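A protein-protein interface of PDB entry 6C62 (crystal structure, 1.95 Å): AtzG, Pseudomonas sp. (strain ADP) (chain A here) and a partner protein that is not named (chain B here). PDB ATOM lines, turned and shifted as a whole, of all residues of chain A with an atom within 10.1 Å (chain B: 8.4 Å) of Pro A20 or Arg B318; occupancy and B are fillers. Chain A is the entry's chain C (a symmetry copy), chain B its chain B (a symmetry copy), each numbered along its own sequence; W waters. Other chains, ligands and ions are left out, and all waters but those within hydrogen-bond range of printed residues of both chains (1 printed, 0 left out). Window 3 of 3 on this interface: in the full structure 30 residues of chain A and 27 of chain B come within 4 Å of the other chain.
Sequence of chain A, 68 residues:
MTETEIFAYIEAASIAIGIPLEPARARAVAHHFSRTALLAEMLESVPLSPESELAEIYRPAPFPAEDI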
ATOM      1  N   ILE A  10      31.176 -16.465   1.528  1.00  0.00           N
ATOM      2  CA  ILE A  10      31.273 -17.920   1.603  1.00  0.00           C
ATOM      3  C   ILE A  10      31.254 -18.355   3.071  1.00  0.00           C
ATOM      4  O   ILE A  10      30.499 -19.289   3.464  1.00  0.00           O
ATOM      5  CB  ILE A  10      32.587 -18.460   0.917  1.00  0.00           C
ATOM      6  CG1 ILE A  10      32.600 -18.275  -0.597  1.00  0.00           C
ATOM      7  CG2 ILE A  10      32.801 -19.942   1.192  1.00  0.00           C
ATOM      8  CD1 ILE A  10      31.336 -18.503  -1.345  1.00  0.00           C
ATOM      9  N   GLU A  11      32.062 -17.677   3.900  1.00  0.00           N
ATOM     10  CA  GLU A  11      32.088 -17.983   5.319  1.00  0.00           C
ATOM     11  C   GLU A  11      30.752 -17.794   6.004  1.00  0.00           C
ATOM     12  O   GLU A  11      30.280 -18.698   6.696  1.00  0.00           O
ATOM     13  CB  GLU A  11      33.140 -17.141   6.046  1.00  0.00           C
ATOM     14  CG  GLU A  11      34.546 -17.569   5.641  1.00  0.00           C
ATOM     15  CD  GLU A  11      35.624 -17.085   6.632  1.00  0.00           C
ATOM     16  OE1 GLU A  11      35.700 -15.850   6.956  1.00  0.00           O
ATOM     17  OE2 GLU A  11      36.388 -17.979   7.080  1.00  0.00           O
ATOM     18  N   ALA A  12      30.122 -16.633   5.792  1.00  0.00           N
ATOM     19  CA  ALA A  12      28.847 -16.343   6.462  1.00  0.00           C
ATOM     20  C   ALA A  12      27.713 -17.183   5.903  1.00  0.00           C
ATOM     21  O   ALA A  12      26.830 -17.616   6.667  1.00  0.00           O
ATOM     22  CB  ALA A  12      28.545 -14.849   6.401  1.00  0.00           C
ATOM     23  N   ALA A  13      27.671 -17.348   4.592  1.00  0.00           N
ATOM     24  CA  ALA A  13      26.574 -18.110   3.958  1.00  0.00           C
ATOM     25  C   ALA A  13      26.605 -19.622   4.327  1.00  0.00           C
ATOM     26  O   ALA A  13      25.558 -20.253   4.563  1.00  0.00           O
ATOM     27  CB  ALA A  13      26.578 -17.962   2.464  1.00  0.00           C
ATOM     28  N   SER A  14      27.810 -20.160   4.418  1.00  0.00           N
ATOM     29  CA  SER A  14      27.999 -21.580   4.760  1.00  0.00           C
ATOM     30  C   SER A  14      27.547 -21.793   6.204  1.00  0.00           C
ATOM     31  O   SER A  14      26.792 -22.728   6.479  1.00  0.00           O
ATOM     32  CB  SER A  14      29.440 -22.089   4.492  1.00  0.00           C
ATOM     33  OG  SER A  14      30.347 -21.427   5.353  1.00  0.00           O
ATOM     34  N   ILE A  15      27.959 -20.914   7.111  1.00  0.00           N
ATOM     35  CA  ILE A  15      27.458 -20.980   8.516  1.00  0.00           C
ATOM     36  C   ILE A  15      25.938 -20.864   8.567  1.00  0.00           C
ATOM     37  O   ILE A  15      25.299 -21.687   9.210  1.00  0.00           O
ATOM     38  CB  ILE A  15      28.123 -19.911   9.428  1.00  0.00           C
ATOM     39  CG1 ILE A  15      29.585 -20.283   9.646  1.00  0.00           C
ATOM     40  CG2 ILE A  15      27.371 -19.791  10.770  1.00  0.00           C
ATOM     41  CD1 ILE A  15      30.446 -19.135  10.170  1.00  0.00           C
ATOM     42  N   ALA A  16      25.361 -19.903   7.848  1.00  0.00           N
ATOM     43  CA  ALA A  16      23.922 -19.712   7.860  1.00  0.00           C
ATOM     44  C   ALA A  16      23.112 -20.940   7.424  1.00  0.00           C
ATOM     45  O   ALA A  16      22.019 -21.173   7.940  1.00  0.00           O
ATOM     46  CB  ALA A  16      23.534 -18.534   6.962  1.00  0.00           C
ATOM     47  N   ILE A  17      23.576 -21.656   6.410  1.00  0.00           N
ATOM     48  CA  ILE A  17      22.811 -22.768   5.889  1.00  0.00           C
ATOM     49  C   ILE A  17      23.221 -24.090   6.605  1.00  0.00           C
ATOM     50  O   ILE A  17      22.601 -25.118   6.412  1.00  0.00           O
ATOM     51  CB  ILE A  17      22.910 -22.847   4.350  1.00  0.00           C
ATOM     52  CG1 ILE A  17      21.750 -23.605   3.715  1.00  0.00           C
ATOM     53  CG2 ILE A  17      24.210 -23.478   3.928  1.00  0.00           C
ATOM     54  CD1 ILE A  17      20.380 -22.980   3.936  1.00  0.00           C
ATOM     55  N   GLY A  18      24.244 -24.065   7.443  1.00  0.00           N
ATOM     56  CA  GLY A  18      24.638 -25.256   8.223  1.00  0.00           C
ATOM     57  C   GLY A  18      25.725 -26.138   7.603  1.00  0.00           C
ATOM     58  O   GLY A  18      25.902 -27.273   8.026  1.00  0.00           O
ATOM     59  N   ILE A  19      26.526 -25.609   6.674  1.00  0.00           N
ATOM     60  CA  ILE A  19      27.582 -26.388   6.046  1.00  0.00           C
ATOM     61  C   ILE A  19      28.901 -25.932   6.646  1.00  0.00           C
ATOM     62  O   ILE A  19      29.432 -24.909   6.236  1.00  0.00           O
ATOM     63  CB  ILE A  19      27.623 -26.306   4.514  1.00  0.00           C
ATOM     64  CG1 ILE A  19      26.340 -26.864   3.918  1.00  0.00           C
ATOM     65  CG2 ILE A  19      28.820 -27.102   3.996  1.00  0.00           C
ATOM     66  CD1 ILE A  19      26.159 -26.481   2.449  1.00  0.00           C
ATOM     67  N   PRO A  20      29.492 -26.770   7.519  1.00  0.00           N
ATOM     68  CA  PRO A  20      30.746 -26.398   8.211  1.00  0.00           C
ATOM     69  C   PRO A  20      31.922 -26.410   7.233  1.00  0.00           C
ATOM     70  O   PRO A  20      32.112 -27.465   6.561  1.00  0.00           O
ATOM     71  CB  PRO A  20      30.939 -27.574   9.202  1.00  0.00           C
ATOM     72  CG  PRO A  20      30.321 -28.782   8.507  1.00  0.00           C
ATOM     73  CD  PRO A  20      29.252 -28.252   7.551  1.00  0.00           C
ATOM     74  N   LEU A  21      32.648 -25.310   7.114  1.00  0.00           N
ATOM     75  CA  LEU A  21      33.780 -25.201   6.216  1.00  0.00           C
ATOM     76  C   LEU A  21      35.090 -24.856   6.946  1.00  0.00           C
ATOM     77  O   LEU A  21      35.252 -23.744   7.418  1.00  0.00           O
ATOM     78  CB  LEU A  21      33.552 -24.135   5.092  1.00  0.00           C
ATOM     79  CG  LEU A  21      32.398 -24.368   4.105  1.00  0.00           C
ATOM     80  CD1 LEU A  21      32.401 -23.337   3.023  1.00  0.00           C
ATOM     81  CD2 LEU A  21      32.447 -25.712   3.430  1.00  0.00           C
ATOM     82  N   GLU A  22      36.052 -25.766   6.916  1.00  0.00           N
ATOM     83  CA  GLU A  22      37.435 -25.465   7.325  1.00  0.00           C
ATOM     84  C   GLU A  22      38.055 -24.456   6.326  1.00  0.00           C
ATOM     85  O   GLU A  22      37.576 -24.334   5.191  1.00  0.00           O
ATOM     86  CB  GLU A  22      38.292 -26.740   7.314  1.00  0.00           C
ATOM     87  CG  GLU A  22      37.920 -27.856   8.273  1.00  0.00           C
ATOM     88  CD  GLU A  22      37.815 -27.433   9.737  1.00  0.00           C
ATOM     89  OE1 GLU A  22      38.722 -26.740  10.256  1.00  0.00           O
ATOM     90  OE2 GLU A  22      36.812 -27.831  10.391  1.00  0.00           O
ATOM     91  N   PRO A  23      39.120 -23.734   6.738  1.00  0.00           N
ATOM     92  CA  PRO A  23      39.729 -22.744   5.854  1.00  0.00           C
ATOM     93  C   PRO A  23      40.157 -23.242   4.447  1.00  0.00           C
ATOM     94  O   PRO A  23      39.873 -22.563   3.482  1.00  0.00           O
ATOM     95  CB  PRO A  23      40.915 -22.230   6.679  1.00  0.00           C
ATOM     96  CG  PRO A  23      40.405 -22.317   8.076  1.00  0.00           C
ATOM     97  CD  PRO A  23      39.606 -23.597   8.129  1.00  0.00           C
ATOM     98  N   ALA A  24      40.777 -24.403   4.312  1.00  0.00           N
ATOM     99  CA  ALA A  24      41.171 -24.882   2.983  1.00  0.00           C
ATOM    100  C   ALA A  24      39.891 -25.160   2.139  1.00  0.00           C
ATOM    101  O   ALA A  24      39.849 -24.846   0.923  1.00  0.00           O
ATOM    102  CB  ALA A  24      41.996 -26.149   3.089  1.00  0.00           C
ATOM    103  N   ARG A  25      38.842 -25.710   2.784  1.00  0.00           N
ATOM    104  CA  ARG A  25      37.629 -25.963   2.056  1.00  0.00           C
ATOM    105  C   ARG A  25      36.967 -24.664   1.631  1.00  0.00           C
ATOM    106  O   ARG A  25      36.532 -24.553   0.493  1.00  0.00           O
ATOM    107  CB  ARG A  25      36.664 -26.913   2.774  1.00  0.00           C
ATOM    108  CG  ARG A  25      35.556 -27.348   1.819  1.00  0.00           C
ATOM    109  CD  ARG A  25      34.492 -28.315   2.368  1.00  0.00           C
ATOM    110  NE  ARG A  25      34.969 -29.600   2.847  1.00  0.00           N
ATOM    111  CZ  ARG A  25      35.524 -30.551   2.106  1.00  0.00           C
ATOM    112  NH1 ARG A  25      35.722 -30.431   0.810  1.00  0.00           N
ATOM    113  NH2 ARG A  25      35.870 -31.672   2.692  1.00  0.00           N
ATOM    114  N   ALA A  26      36.943 -23.672   2.506  1.00  0.00           N
ATOM    115  CA  ALA A  26      36.351 -22.381   2.133  1.00  0.00           C
ATOM    116  C   ALA A  26      37.053 -21.756   0.928  1.00  0.00           C
ATOM    117  O   ALA A  26      36.383 -21.207   0.051  1.00  0.00           O
ATOM    118  CB  ALA A  26      36.357 -21.435   3.312  1.00  0.00           C
ATOM    119  N   VAL A  29      35.886 -23.686  -2.185  1.00  0.00           N
ATOM    120  CA  VAL A  29      34.558 -23.240  -2.501  1.00  0.00           C
ATOM    121  C   VAL A  29      34.568 -21.828  -3.153  1.00  0.00           C
ATOM    122  O   VAL A  29      33.901 -21.619  -4.171  1.00  0.00           O
ATOM    123  CB  VAL A  29      33.614 -23.338  -1.277  1.00  0.00           C
ATOM    124  CG1 VAL A  29      32.293 -22.649  -1.579  1.00  0.00           C
ATOM    125  CG2 VAL A  29      33.442 -24.819  -0.890  1.00  0.00           C
ATOM    126  N   GLY B 310      23.196 -28.934  -5.923  1.00  0.00           N
ATOM    127  CA  GLY B 310      23.685 -28.765  -4.585  1.00  0.00           C
ATOM    128  C   GLY B 310      22.606 -28.829  -3.512  1.00  0.00           C
ATOM    129  O   GLY B 310      22.788 -29.523  -2.465  1.00  0.00           O
ATOM    130  N   CYS B 311      21.492 -28.116  -3.713  1.00  0.00           N
ATOM    131  CA  CYS B 311      20.432 -28.146  -2.691  1.00  0.00           C
ATOM    132  C   CYS B 311      19.797 -29.522  -2.522  1.00  0.00           C
ATOM    133  O   CYS B 311      19.370 -29.886  -1.454  1.00  0.00           O
ATOM    134  CB  CYS B 311      19.387 -27.086  -2.942  1.00  0.00           C
ATOM    135  SG  CYS B 311      20.190 -25.399  -2.743  1.00  0.00           S
ATOM    136  N   HIS B 313      21.311 -32.172  -2.246  1.00  0.00           N
ATOM    137  CA  HIS B 313      22.205 -32.924  -1.358  1.00  0.00           C
ATOM    138  C   HIS B 313      22.498 -32.194  -0.040  1.00  0.00           C
ATOM    139  O   HIS B 313      23.439 -32.540   0.675  1.00  0.00           O
ATOM    140  CB  HIS B 313      23.510 -33.207  -2.112  1.00  0.00           C
ATOM    141  CG  HIS B 313      23.320 -34.127  -3.267  1.00  0.00           C
ATOM    142  ND1 HIS B 313      23.077 -35.468  -3.096  1.00  0.00           N
ATOM    143  CD2 HIS B 313      23.257 -33.903  -4.596  1.00  0.00           C
ATOM    144  CE1 HIS B 313      22.897 -36.032  -4.272  1.00  0.00           C
ATOM    145  NE2 HIS B 313      22.994 -35.105  -5.202  1.00  0.00           N
ATOM    146  N   LEU B 314      21.696 -31.192   0.290  1.00  0.00           N
ATOM    147  CA  LEU B 314      22.029 -30.323   1.399  1.00  0.00           C
ATOM    148  C   LEU B 314      22.146 -31.037   2.751  1.00  0.00           C
ATOM    149  O   LEU B 314      23.045 -30.744   3.515  1.00  0.00           O
ATOM    150  CB  LEU B 314      21.056 -29.142   1.461  1.00  0.00           C
ATOM    151  CG  LEU B 314      21.228 -28.155   2.579  1.00  0.00           C
ATOM    152  CD1 LEU B 314      22.592 -27.521   2.571  1.00  0.00           C
ATOM    153  CD2 LEU B 314      20.171 -27.046   2.460  1.00  0.00           C
ATOM    154  N   ASP B 315      21.281 -31.982   3.026  1.00  0.00           N
ATOM    155  CA  ASP B 315      21.331 -32.670   4.316  1.00  0.00           C
ATOM    156  C   ASP B 315      22.580 -33.443   4.506  1.00  0.00           C
ATOM    157  O   ASP B 315      23.169 -33.389   5.590  1.00  0.00           O
ATOM    158  CB  ASP B 315      20.090 -33.519   4.603  1.00  0.00           C
ATOM    159  CG  ASP B 315      18.858 -32.624   4.979  1.00  0.00           C
ATOM    160  OD1 ASP B 315      19.020 -31.570   5.692  1.00  0.00           O
ATOM    161  OD2 ASP B 315      17.718 -32.968   4.599  1.00  0.00           O
ATOM    162  N   ASP B 316      23.027 -34.130   3.467  1.00  0.00           N
ATOM    163  CA  ASP B 316      24.344 -34.761   3.506  1.00  0.00           C
ATOM    164  C   ASP B 316      25.527 -33.804   3.502  1.00  0.00           C
ATOM    165  O   ASP B 316      26.549 -34.051   4.158  1.00  0.00           O
ATOM    166  CB  ASP B 316      24.428 -35.803   2.391  1.00  0.00           C
ATOM    167  CG  ASP B 316      23.656 -37.049   2.716  1.00  0.00           C
ATOM    168  OD1 ASP B 316      23.656 -37.398   3.896  1.00  0.00           O
ATOM    169  OD2 ASP B 316      23.056 -37.683   1.794  1.00  0.00           O
ATOM    170  N   LEU B 317      25.406 -32.687   2.789  1.00  0.00           N
ATOM    171  CA  LEU B 317      26.498 -31.718   2.853  1.00  0.00           C
ATOM    172  C   LEU B 317      26.647 -31.101   4.228  1.00  0.00           C
ATOM    173  O   LEU B 317      27.768 -30.703   4.611  1.00  0.00           O
ATOM    174  CB  LEU B 317      26.332 -30.627   1.782  1.00  0.00           C
ATOM    175  CG  LEU B 317      26.453 -31.066   0.314  1.00  0.00           C
ATOM    176  CD1 LEU B 317      25.938 -29.922  -0.571  1.00  0.00           C
ATOM    177  CD2 LEU B 317      27.867 -31.377  -0.035  1.00  0.00           C
ATOM    178  N   ARG B 318      25.561 -31.035   4.996  1.00  0.00           N
ATOM    179  CA  ARG B 318      25.604 -30.549   6.344  1.00  0.00           C
ATOM    180  C   ARG B 318      26.351 -31.452   7.318  1.00  0.00           C
ATOM    181  O   ARG B 318      27.087 -30.935   8.191  1.00  0.00           O
ATOM    182  CB  ARG B 318      24.210 -30.278   6.898  1.00  0.00           C
ATOM    183  CG  ARG B 318      23.544 -29.064   6.321  1.00  0.00           C
ATOM    184  CD  ARG B 318      22.088 -29.055   6.632  1.00  0.00           C
ATOM    185  NE  ARG B 318      21.516 -27.738   6.426  1.00  0.00           N
ATOM    186  CZ  ARG B 318      20.223 -27.487   6.239  1.00  0.00           C
ATOM    187  NH1 ARG B 318      19.350 -28.449   6.154  1.00  0.00           N
ATOM    188  NH2 ARG B 318      19.797 -26.267   6.064  1.00  0.00           N
ATOM    189  N   ILE B 319      26.183 -32.751   7.219  1.00  0.00           N
ATOM    190  CA  ILE B 319      26.776 -33.619   8.212  1.00  0.00           C
ATOM    191  C   ILE B 319      28.034 -34.357   7.725  1.00  0.00           C
ATOM    192  O   ILE B 319      28.895 -34.669   8.567  1.00  0.00           O
ATOM    193  CB  ILE B 319      25.731 -34.608   8.744  1.00  0.00           C
ATOM    194  CG1 ILE B 319      26.189 -35.274  10.065  1.00  0.00           C
ATOM    195  CG2 ILE B 319      25.340 -35.621   7.656  1.00  0.00           C
ATOM    196  CD1 ILE B 319      26.438 -34.411  11.302  1.00  0.00           C
ATOM    197  N   ARG B 320      28.166 -34.631   6.408  1.00  0.00           N
ATOM    198  CA  ARG B 320      29.262 -35.488   5.919  1.00  0.00           C
ATOM    199  C   ARG B 320      29.908 -35.099   4.611  1.00  0.00           C
ATOM    200  O   ARG B 320      30.099 -35.941   3.715  1.00  0.00           O
ATOM    201  CB  ARG B 320      28.805 -36.944   5.889  1.00  0.00           C
ATOM    202  CG  ARG B 320      27.625 -37.208   4.953  1.00  0.00           C
ATOM    203  CD  ARG B 320      26.885 -38.537   5.217  1.00  0.00           C
ATOM    204  NE  ARG B 320      27.777 -39.671   5.040  1.00  0.00           N
ATOM    205  CZ  ARG B 320      27.381 -40.939   4.846  1.00  0.00           C
ATOM    206  NH1 ARG B 320      28.318 -41.872   4.672  1.00  0.00           N
ATOM    207  NH2 ARG B 320      26.100 -41.265   4.831  1.00  0.00           N
ATOM    208  N   PRO B 321      30.372 -33.837   4.515  1.00  0.00           N
ATOM    209  CA  PRO B 321      30.953 -33.403   3.247  1.00  0.00           C
ATOM    210  C   PRO B 321      32.198 -34.206   2.818  1.00  0.00           C
ATOM    211  O   PRO B 321      32.517 -34.352   1.628  1.00  0.00           O
ATOM    212  CB  PRO B 321      31.305 -31.911   3.524  1.00  0.00           C
ATOM    213  CG  PRO B 321      31.379 -31.819   4.996  1.00  0.00           C
ATOM    214  CD  PRO B 321      30.392 -32.791   5.548  1.00  0.00           C
ATOM    215  N   GLN B 322      32.938 -34.684   3.804  1.00  0.00           N
ATOM    216  CA  GLN B 322      34.115 -35.523   3.560  1.00  0.00           C
ATOM    217  C   GLN B 322      33.832 -36.890   2.888  1.00  0.00           C
ATOM    218  O   GLN B 322      34.762 -37.504   2.360  1.00  0.00           O
ATOM    219  CB  GLN B 322      34.880 -35.768   4.872  1.00  0.00           C
ATOM    220  CG  GLN B 322      34.239 -36.764   5.798  1.00  0.00           C
ATOM    221  CD  GLN B 322      33.149 -36.198   6.682  1.00  0.00           C
ATOM    222  OE1 GLN B 322      32.748 -34.948   6.647  1.00  0.00           O
ATOM    223  NE2 GLN B 322      32.622 -37.111   7.488  1.00  0.00           N
ATOM    224  N   PHE B 324      31.678 -37.171   0.298  1.00  0.00           N
ATOM    225  CA  PHE B 324      31.380 -36.952  -1.118  1.00  0.00           C
ATOM    226  C   PHE B 324      32.715 -37.095  -1.919  1.00  0.00           C
ATOM    227  O   PHE B 324      33.831 -37.119  -1.367  1.00  0.00           O
ATOM    228  CB  PHE B 324      30.857 -35.526  -1.334  1.00  0.00           C
ATOM    229  CG  PHE B 324      29.441 -35.279  -0.917  1.00  0.00           C
ATOM    230  CD1 PHE B 324      29.078 -35.242   0.416  1.00  0.00           C
ATOM    231  CD2 PHE B 324      28.462 -35.044  -1.881  1.00  0.00           C
ATOM    232  CE1 PHE B 324      27.758 -34.987   0.770  1.00  0.00           C
ATOM    233  CE2 PHE B 324      27.161 -34.835  -1.538  1.00  0.00           C
ATOM    234  CZ  PHE B 324      26.801 -34.813  -0.237  1.00  0.00           C
ATOM    235  N   ASP B 330      33.058 -29.455  -3.495  1.00  0.00           N
ATOM    236  CA  ASP B 330      33.143 -27.995  -3.369  1.00  0.00           C
ATOM    237  C   ASP B 330      32.333 -27.275  -4.434  1.00  0.00           C
ATOM    238  O   ASP B 330      31.876 -26.158  -4.199  1.00  0.00           O
ATOM    239  CB  ASP B 330      34.576 -27.495  -3.329  1.00  0.00           C
ATOM    240  CG  ASP B 330      35.389 -28.169  -2.195  1.00  0.00           C
ATOM    241  OD1 ASP B 330      34.766 -28.418  -1.122  1.00  0.00           O
ATOM    242  OD2 ASP B 330      36.588 -28.530  -2.406  1.00  0.00           O
ATOM    243  N   ILE B 333      28.831 -27.436  -2.982  1.00  0.00           N
ATOM    244  CA  ILE B 333      28.705 -26.458  -1.924  1.00  0.00           C
ATOM    245  C   ILE B 333      28.580 -25.030  -2.501  1.00  0.00           C
ATOM    246  O   ILE B 333      27.726 -24.243  -2.095  1.00  0.00           O
ATOM    247  CB  ILE B 333      29.847 -26.563  -0.922  1.00  0.00           C
ATOM    248  CG1 ILE B 333      29.732 -27.871  -0.111  1.00  0.00           C
ATOM    249  CG2 ILE B 333      29.796 -25.382   0.053  1.00  0.00           C
ATOM    250  CD1 ILE B 333      30.974 -28.221   0.670  1.00  0.00           C
ATOM    251  N   VAL B 336      25.043 -24.447  -3.560  1.00  0.00           N
ATOM    252  CA  VAL B 336      24.115 -24.162  -2.429  1.00  0.00           C
ATOM    253  C   VAL B 336      24.206 -22.676  -1.991  1.00  0.00           C
ATOM    254  O   VAL B 336      23.198 -22.101  -1.530  1.00  0.00           O
ATOM    255  CB  VAL B 336      24.460 -25.028  -1.237  1.00  0.00           C
ATOM    256  CG1 VAL B 336      23.682 -24.622  -0.022  1.00  0.00           C
ATOM    257  CG2 VAL B 336      24.135 -26.457  -1.517  1.00  0.00           C
HETATM  258  O   HOH W   1      38.363 -28.599  -0.368  1.00  0.00           O
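Of the 18 printed residues of chain A, 6 touch a printed residue of chain B.
Printed residues of chain A that touch a printed residue of chain B: Ile A17, Gly A18, Ile A19, Pro A20, Arg A25 and Val A29.
Hydrophobic or aromatic side chains of chain A that line the printed part of chain B: Ile A17, Ile A19, Pro A20 and Val A29.
Along chain A the printed residues that touch a printed residue of chain B span positions 17 to 29.
Among the printed residues, 11 pairs touch across the chains.
Leu B314 touches Ile A17 (CD2 to CG1, 3.99 Å).
O of Gly A18 touches CG of Arg B318 (3.4 Å).
CD1 of Leu B314 touches CD1 of Ile A19, 3.7 Å away.
CG2 of Ile A19 touches O of Leu B317 (3.8 Å).
Ile A19 touches Val B336 (CD1 to CG1, 3.96 Å).
Pro A20 touches Arg B318.
Arg A25 touches Ile B333.
CG2 of Val A29 touches CB of Asp B330 (3.8 Å).
Ile B333 touches Val A29 (CG2 to CG2, 3.8 Å).
Pro A20 touches just one residue of chain B: Arg B318.
Of the printed residues of chain A, Arg B318 touches Ile A17 (2.8 Å), Gly A18 (3.4 Å) and Pro A20 (3.5 Å).
No residue of chain A comes within 4 Å of Asp B315.
Of chain A, only Ile A19 (3.8 Å) comes within 4 Å of Leu B317.
Ile B319 touches none of the printed residues of chain A.
Of the printed residues of chain B, Ile A17 touches Leu B314 (3.99 Å) and Arg B318 (2.8 Å).
Of the printed residues of chain B, Ile A19 touches Leu B314 (3.7 Å), Leu B317 (3.8 Å) and Val B336 (3.96 Å).
Of the printed residues of chain A, Asp B330 touches Arg A25 (2.9 Å) and Val A29 (3.8 Å).
Of the printed residues of chain B, Gly A18 touches Arg B318 (3.4 Å).
Of the printed residues of chain A, Ile B333 touches Arg A25 and Val A29.
The nearest residue of chain B that does not touch Pro A20 is Leu B317 (4.1 Å).
Water W1 bridges the side-chain carboxylate of Asp B330 and the guanidinium group of Arg A25.
The side-chain carboxylate of Asp B315 is in salt-bridge range of the guanidinium group of Arg B318 (3.2 Å).
O of Ser A14 lies within hydrogen-bond range of N of Ile A19 (2.9 Å).
O of Ile A17 lies within hydrogen-bond range of NE of Arg B318, at 2.8 Å.
The side-chain carboxylate of Asp B330 is in salt-bridge range of the guanidinium group of Arg A25 (2.9 Å).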
